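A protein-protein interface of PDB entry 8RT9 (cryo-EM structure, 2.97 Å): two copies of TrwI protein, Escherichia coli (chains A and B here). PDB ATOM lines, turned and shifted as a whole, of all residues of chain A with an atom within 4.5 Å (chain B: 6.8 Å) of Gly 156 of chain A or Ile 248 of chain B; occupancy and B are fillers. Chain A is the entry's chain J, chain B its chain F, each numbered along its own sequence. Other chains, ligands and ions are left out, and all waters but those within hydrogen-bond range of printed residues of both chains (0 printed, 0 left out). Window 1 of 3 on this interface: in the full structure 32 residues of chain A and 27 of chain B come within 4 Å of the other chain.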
ATOM      1  N   PHE A   3     -21.417  -0.042   9.908  1.00  0.00           N
ATOM      2  CA  PHE A   3     -20.393  -1.045  10.171  1.00  0.00           C
ATOM      3  C   PHE A   3     -21.019  -2.178  10.967  1.00  0.00           C
ATOM      4  O   PHE A   3     -21.414  -1.993  12.120  1.00  0.00           O
ATOM      5  CB  PHE A   3     -19.220  -0.432  10.924  1.00  0.00           C
ATOM      6  CG  PHE A   3     -18.116  -1.396  11.209  1.00  0.00           C
ATOM      7  CD1 PHE A   3     -17.168  -1.675  10.259  1.00  0.00           C
ATOM      8  CD2 PHE A   3     -18.024  -2.016  12.433  1.00  0.00           C
ATOM      9  CE1 PHE A   3     -16.157  -2.555  10.519  1.00  0.00           C
ATOM     10  CE2 PHE A   3     -17.010  -2.898  12.696  1.00  0.00           C
ATOM     11  CZ  PHE A   3     -16.077  -3.166  11.737  1.00  0.00           C
ATOM     12  N   LEU A   5     -19.799  -5.959  11.631  1.00  0.00           N
ATOM     13  CA  LEU A   5     -18.877  -7.076  11.505  1.00  0.00           C
ATOM     14  C   LEU A   5     -19.004  -8.086  12.628  1.00  0.00           C
ATOM     15  O   LEU A   5     -19.017  -9.289  12.366  1.00  0.00           O
ATOM     16  CB  LEU A   5     -17.438  -6.572  11.447  1.00  0.00           C
ATOM     17  CG  LEU A   5     -16.416  -7.666  11.168  1.00  0.00           C
ATOM     18  CD1 LEU A   5     -16.324  -7.931   9.683  1.00  0.00           C
ATOM     19  CD2 LEU A   5     -15.075  -7.266  11.712  1.00  0.00           C
ATOM     20  N   PHE A   6     -19.096  -7.630  13.874  1.00  0.00           N
ATOM     21  CA  PHE A   6     -19.136  -8.564  14.989  1.00  0.00           C
ATOM     22  C   PHE A   6     -20.494  -9.227  15.141  1.00  0.00           C
ATOM     23  O   PHE A   6     -20.561 -10.378  15.581  1.00  0.00           O
ATOM     24  CB  PHE A   6     -18.736  -7.856  16.277  1.00  0.00           C
ATOM     25  CG  PHE A   6     -17.260  -7.775  16.473  1.00  0.00           C
ATOM     26  CD1 PHE A   6     -16.558  -8.855  16.959  1.00  0.00           C
ATOM     27  CD2 PHE A   6     -16.570  -6.629  16.150  1.00  0.00           C
ATOM     28  CE1 PHE A   6     -15.200  -8.790  17.131  1.00  0.00           C
ATOM     29  CE2 PHE A   6     -15.209  -6.559  16.322  1.00  0.00           C
ATOM     30  CZ  PHE A   6     -14.523  -7.642  16.814  1.00  0.00           C
ATOM     31  N   PHE A 124     -13.344   3.800  12.531  1.00  0.00           N
ATOM     32  CA  PHE A 124     -13.190   3.640  11.096  1.00  0.00           C
ATOM     33  C   PHE A 124     -13.739   4.834  10.336  1.00  0.00           C
ATOM     34  O   PHE A 124     -13.259   5.142   9.245  1.00  0.00           O
ATOM     35  CB  PHE A 124     -13.863   2.352  10.642  1.00  0.00           C
ATOM     36  CG  PHE A 124     -13.185   1.118  11.137  1.00  0.00           C
ATOM     37  CD1 PHE A 124     -11.834   1.122  11.402  1.00  0.00           C
ATOM     38  CD2 PHE A 124     -13.890  -0.044  11.333  1.00  0.00           C
ATOM     39  CE1 PHE A 124     -11.207  -0.007  11.855  1.00  0.00           C
ATOM     40  CE2 PHE A 124     -13.263  -1.173  11.787  1.00  0.00           C
ATOM     41  CZ  PHE A 124     -11.921  -1.153  12.048  1.00  0.00           C
ATOM     42  N   LEU A 152      -6.967   3.220  11.735  1.00  0.00           N
ATOM     43  CA  LEU A 152      -7.577   1.954  11.366  1.00  0.00           C
ATOM     44  C   LEU A 152      -6.936   0.801  12.116  1.00  0.00           C
ATOM     45  O   LEU A 152      -7.634  -0.070  12.640  1.00  0.00           O
ATOM     46  CB  LEU A 152      -7.450   1.758   9.857  1.00  0.00           C
ATOM     47  CG  LEU A 152      -8.128   0.583   9.169  1.00  0.00           C
ATOM     48  CD1 LEU A 152      -8.758   1.057   7.883  1.00  0.00           C
ATOM     49  CD2 LEU A 152      -7.123  -0.509   8.888  1.00  0.00           C
ATOM     50  N   LEU A 153      -5.607   0.792  12.196  1.00  0.00           N
ATOM     51  CA  LEU A 153      -4.916  -0.288  12.883  1.00  0.00           C
ATOM     52  C   LEU A 153      -5.205  -0.271  14.376  1.00  0.00           C
ATOM     53  O   LEU A 153      -5.451  -1.321  14.969  1.00  0.00           O
ATOM     54  CB  LEU A 153      -3.418  -0.201  12.624  1.00  0.00           C
ATOM     55  CG  LEU A 153      -2.978  -0.740  11.266  1.00  0.00           C
ATOM     56  CD1 LEU A 153      -1.492  -0.522  11.064  1.00  0.00           C
ATOM     57  CD2 LEU A 153      -3.328  -2.204  11.143  1.00  0.00           C
ATOM     58  N   ALA A 154      -5.188   0.901  15.006  1.00  0.00           N
ATOM     59  CA  ALA A 154      -5.479   0.955  16.435  1.00  0.00           C
ATOM     60  C   ALA A 154      -6.868   0.406  16.728  1.00  0.00           C
ATOM     61  O   ALA A 154      -7.039  -0.490  17.574  1.00  0.00           O
ATOM     62  CB  ALA A 154      -5.347   2.388  16.939  1.00  0.00           C
ATOM     63  N   THR A 155      -7.872   0.909  16.005  1.00  0.00           N
ATOM     64  CA  THR A 155      -9.239   0.450  16.218  1.00  0.00           C
ATOM     65  C   THR A 155      -9.362  -1.045  15.959  1.00  0.00           C
ATOM     66  O   THR A 155      -9.966  -1.779  16.752  1.00  0.00           O
ATOM     67  CB  THR A 155     -10.191   1.227  15.315  1.00  0.00           C
ATOM     68  OG1 THR A 155     -10.065   2.627  15.584  1.00  0.00           O
ATOM     69  CG2 THR A 155     -11.613   0.802  15.572  1.00  0.00           C
ATOM     70  N   GLY A 156      -8.783  -1.515  14.854  1.00  0.00           N
ATOM     71  CA  GLY A 156      -8.928  -2.910  14.492  1.00  0.00           C
ATOM     72  C   GLY A 156      -8.255  -3.847  15.469  1.00  0.00           C
ATOM     73  O   GLY A 156      -8.825  -4.866  15.848  1.00  0.00           O
ATOM     74  N   LEU A 157      -7.029  -3.522  15.885  1.00  0.00           N
ATOM     75  CA  LEU A 157      -6.356  -4.333  16.892  1.00  0.00           C
ATOM     76  C   LEU A 157      -7.162  -4.415  18.177  1.00  0.00           C
ATOM     77  O   LEU A 157      -7.381  -5.516  18.700  1.00  0.00           O
ATOM     78  CB  LEU A 157      -4.951  -3.793  17.172  1.00  0.00           C
ATOM     79  CG  LEU A 157      -3.731  -4.155  16.312  1.00  0.00           C
ATOM     80  CD1 LEU A 157      -3.478  -5.637  16.460  1.00  0.00           C
ATOM     81  CD2 LEU A 157      -3.878  -3.823  14.837  1.00  0.00           C
ATOM     82  N   LEU A 158      -7.631  -3.280  18.694  1.00  0.00           N
ATOM     83  CA  LEU A 158      -8.368  -3.332  19.952  1.00  0.00           C
ATOM     84  C   LEU A 158      -9.627  -4.180  19.815  1.00  0.00           C
ATOM     85  O   LEU A 158      -9.863  -5.114  20.604  1.00  0.00           O
ATOM     86  CB  LEU A 158      -8.706  -1.919  20.416  1.00  0.00           C
ATOM     87  CG  LEU A 158      -9.657  -1.804  21.598  1.00  0.00           C
ATOM     88  CD1 LEU A 158      -9.145  -2.616  22.760  1.00  0.00           C
ATOM     89  CD2 LEU A 158      -9.802  -0.357  21.995  1.00  0.00           C
ATOM     90  N   ALA A 159     -10.438  -3.886  18.794  1.00  0.00           N
ATOM     91  CA  ALA A 159     -11.691  -4.604  18.623  1.00  0.00           C
ATOM     92  C   ALA A 159     -11.452  -6.083  18.386  1.00  0.00           C
ATOM     93  O   ALA A 159     -12.163  -6.929  18.937  1.00  0.00           O
ATOM     94  CB  ALA A 159     -12.489  -3.999  17.473  1.00  0.00           C
ATOM     95  N   ALA A 160     -10.458  -6.419  17.567  1.00  0.00           N
ATOM     96  CA  ALA A 160     -10.205  -7.811  17.236  1.00  0.00           C
ATOM     97  C   ALA A 160      -9.760  -8.591  18.458  1.00  0.00           C
ATOM     98  O   ALA A 160     -10.244  -9.700  18.700  1.00  0.00           O
ATOM     99  CB  ALA A 160      -9.160  -7.899  16.126  1.00  0.00           C
ATOM    100  N   ILE B 243     -11.357  -2.404   4.884  1.00  0.00           N
ATOM    101  CA  ILE B 243     -10.013  -2.740   5.343  1.00  0.00           C
ATOM    102  C   ILE B 243     -10.016  -3.043   6.836  1.00  0.00           C
ATOM    103  O   ILE B 243      -9.308  -3.945   7.304  1.00  0.00           O
ATOM    104  CB  ILE B 243      -9.027  -1.611   4.996  1.00  0.00           C
ATOM    105  CG1 ILE B 243      -9.084  -1.293   3.506  1.00  0.00           C
ATOM    106  CG2 ILE B 243      -7.617  -1.996   5.395  1.00  0.00           C
ATOM    107  CD1 ILE B 243      -8.273  -2.221   2.658  1.00  0.00           C
ATOM    108  N   GLY B 244     -10.809  -2.301   7.608  1.00  0.00           N
ATOM    109  CA  GLY B 244     -10.889  -2.569   9.029  1.00  0.00           C
ATOM    110  C   GLY B 244     -11.498  -3.921   9.329  1.00  0.00           C
ATOM    111  O   GLY B 244     -11.030  -4.634  10.217  1.00  0.00           O
ATOM    112  N   GLY B 245     -12.551  -4.290   8.606  1.00  0.00           N
ATOM    113  CA  GLY B 245     -13.099  -5.621   8.768  1.00  0.00           C
ATOM    114  C   GLY B 245     -12.094  -6.695   8.412  1.00  0.00           C
ATOM    115  O   GLY B 245     -12.008  -7.726   9.081  1.00  0.00           O
ATOM    116  N   SER B 246     -11.311  -6.459   7.359  1.00  0.00           N
ATOM    117  CA  SER B 246     -10.269  -7.409   6.989  1.00  0.00           C
ATOM    118  C   SER B 246      -9.274  -7.603   8.124  1.00  0.00           C
ATOM    119  O   SER B 246      -8.967  -8.738   8.508  1.00  0.00           O
ATOM    120  CB  SER B 246      -9.554  -6.932   5.727  1.00  0.00           C
ATOM    121  OG  SER B 246      -8.492  -7.805   5.388  1.00  0.00           O
ATOM    122  N   VAL B 247      -8.766  -6.504   8.684  1.00  0.00           N
ATOM    123  CA  VAL B 247      -7.751  -6.634   9.725  1.00  0.00           C
ATOM    124  C   VAL B 247      -8.351  -7.231  10.991  1.00  0.00           C
ATOM    125  O   VAL B 247      -7.700  -8.024  11.681  1.00  0.00           O
ATOM    126  CB  VAL B 247      -7.046  -5.291   9.998  1.00  0.00           C
ATOM    127  CG1 VAL B 247      -6.409  -4.770   8.735  1.00  0.00           C
ATOM    128  CG2 VAL B 247      -7.994  -4.271  10.575  1.00  0.00           C
ATOM    129  N   ILE B 248      -9.597  -6.886  11.311  1.00  0.00           N
ATOM    130  CA  ILE B 248     -10.229  -7.442  12.500  1.00  0.00           C
ATOM    131  C   ILE B 248     -10.417  -8.944  12.352  1.00  0.00           C
ATOM    132  O   ILE B 248     -10.121  -9.711  13.272  1.00  0.00           O
ATOM    133  CB  ILE B 248     -11.562  -6.737  12.790  1.00  0.00           C
ATOM    134  CG1 ILE B 248     -11.321  -5.301  13.233  1.00  0.00           C
ATOM    135  CG2 ILE B 248     -12.305  -7.467  13.880  1.00  0.00           C
ATOM    136  CD1 ILE B 248     -12.584  -4.554  13.548  1.00  0.00           C
ATOM    137  N   LEU B 249     -10.910  -9.390  11.196  1.00  0.00           N
ATOM    138  CA  LEU B 249     -11.080 -10.822  10.984  1.00  0.00           C
ATOM    139  C   LEU B 249      -9.744 -11.540  11.053  1.00  0.00           C
ATOM    140  O   LEU B 249      -9.624 -12.589  11.703  1.00  0.00           O
ATOM    141  CB  LEU B 249     -11.752 -11.082   9.641  1.00  0.00           C
ATOM    142  CG  LEU B 249     -13.266 -10.920   9.581  1.00  0.00           C
ATOM    143  CD1 LEU B 249     -13.756 -11.214   8.188  1.00  0.00           C
ATOM    144  CD2 LEU B 249     -13.929 -11.838  10.576  1.00  0.00           C
ATOM    145  N   SER B 250      -8.723 -10.978  10.404  1.00  0.00           N
ATOM    146  CA  SER B 250      -7.399 -11.582  10.443  1.00  0.00           C
ATOM    147  C   SER B 250      -6.921 -11.753  11.875  1.00  0.00           C
ATOM    148  O   SER B 250      -6.570 -12.861  12.293  1.00  0.00           O
ATOM    149  CB  SER B 250      -6.418 -10.731   9.647  1.00  0.00           C
ATOM    150  OG  SER B 250      -5.110 -11.265   9.718  1.00  0.00           O
ATOM    151  N   ILE B 251      -6.955 -10.678  12.659  1.00  0.00           N
ATOM    152  CA  ILE B 251      -6.382 -10.707  13.999  1.00  0.00           C
ATOM    153  C   ILE B 251      -7.194 -11.608  14.920  1.00  0.00           C
ATOM    154  O   ILE B 251      -6.631 -12.337  15.749  1.00  0.00           O
ATOM    155  CB  ILE B 251      -6.278  -9.273  14.537  1.00  0.00           C
ATOM    156  CG1 ILE B 251      -5.329  -8.475  13.655  1.00  0.00           C
ATOM    157  CG2 ILE B 251      -5.783  -9.274  15.962  1.00  0.00           C
ATOM    158  CD1 ILE B 251      -5.354  -7.011  13.922  1.00  0.00           C
ATOM    159  N   VAL B 252      -8.523 -11.573  14.798  1.00  0.00           N
ATOM    160  CA  VAL B 252      -9.371 -12.450  15.596  1.00  0.00           C
ATOM    161  C   VAL B 252      -9.006 -13.901  15.340  1.00  0.00           C
ATOM    162  O   VAL B 252      -8.782 -14.684  16.275  1.00  0.00           O
ATOM    163  CB  VAL B 252     -10.854 -12.191  15.282  1.00  0.00           C
ATOM    164  CG1 VAL B 252     -11.699 -13.372  15.703  1.00  0.00           C
ATOM    165  CG2 VAL B 252     -11.332 -10.946  15.964  1.00  0.00           C
ATOM    166  N   SER B 253      -8.928 -14.278  14.063  1.00  0.00           N
ATOM    167  CA  SER B 253      -8.578 -15.648  13.727  1.00  0.00           C
ATOM    168  C   SER B 253      -7.194 -15.996  14.248  1.00  0.00           C
ATOM    169  O   SER B 253      -6.971 -17.103  14.749  1.00  0.00           O
ATOM    170  CB  SER B 253      -8.652 -15.840  12.216  1.00  0.00           C
ATOM    171  OG  SER B 253      -9.938 -15.501  11.732  1.00  0.00           O
ATOM    172  N   ILE B 254      -6.259 -15.052  14.160  1.00  0.00           N
ATOM    173  CA  ILE B 254      -4.885 -15.321  14.559  1.00  0.00           C
ATOM    174  C   ILE B 254      -4.813 -15.645  16.041  1.00  0.00           C
ATOM    175  O   ILE B 254      -4.202 -16.639  16.441  1.00  0.00           O
ATOM    176  CB  ILE B 254      -3.988 -14.126  14.206  1.00  0.00           C
ATOM    177  CG1 ILE B 254      -3.740 -14.075  12.708  1.00  0.00           C
ATOM    178  CG2 ILE B 254      -2.670 -14.233  14.924  1.00  0.00           C
ATOM    179  CD1 ILE B 254      -3.546 -12.669  12.205  1.00  0.00           C
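Of the printed residues of chain B, Leu 5 of chain A touches Gly 245 (3.9 Å) and Ile 248 (3.5 Å).
Printed residues of chain B within 4 Å of Phe 124 of chain A: Gly 244 (3.5 Å) and Ile 248 (3.8 Å).
Of the printed residues of chain B, Leu 152 of chain A touches Ile 243 (3.8 Å) and Gly 244 (3.9 Å).
Gly 156 of chain A touches just one residue of chain B: Ile 248 (3.6 Å).
Of the printed residues of chain B, Ala 160 of chain A touches Ile 248, Ile 251 and Val 252.
Of chain A, only Leu 5 (3.5 Å), Phe 6 (3.7 Å), Phe 124 (3.8 Å), Gly 156 (3.6 Å), Ala 159 (3.97 Å) and Ala 160 (3.5 Å) come within 4 Å of Ile 248 of chain B.
The nearest residue of chain A that does not touch Ile 248 of chain B is Phe 3 of chain A (4.2 Å).
Among the printed residues, pairs that only touch across the chains: Ala 160 of chain A with Val 252 of chain B (3.2 Å), Leu 157 of chain A with Ile 251 of chain B (3.4 Å), Phe 124 of chain A with Gly 244 of chain B (3.5 Å), Ala 160 of chain A with Ile 248 of chain B (3.5 Å), Leu 5 of chain A with Ile 248 of chain B (3.5 Å), Ala 160 of chain A with Ile 251 of chain B (3.6 Å), Gly 156 of chain A with Ile 248 of chain B (3.6 Å), Phe 6 of chain A with Ile 248 of chain B (3.7 Å), Phe 124 of chain A with Ile 248 of chain B (3.8 Å), Leu 152 of chain A with Ile 243 of chain B (3.8 Å), Leu 5 of chain A with Gly 245 of chain B (3.9 Å), Leu 152 of chain A with Gly 244 of chain B (3.9 Å) and Ala 159 of chain A with Ile 248 of chain B (3.97 Å).
Hydrophobic or aromatic side chains of chain A that line the printed part of chain B: Leu 5, Phe 6, Phe 124, Leu 152, Leu 157, Ala 159 and Ala 160.
Hydrophobic or aromatic side chains of chain B within 4 Å of the printed part of chain A: Ile 243, Ile 248, Ile 251 and Val 252.
Among the printed residues, 13 pairs touch across the chains.
No position is printed for both chains.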
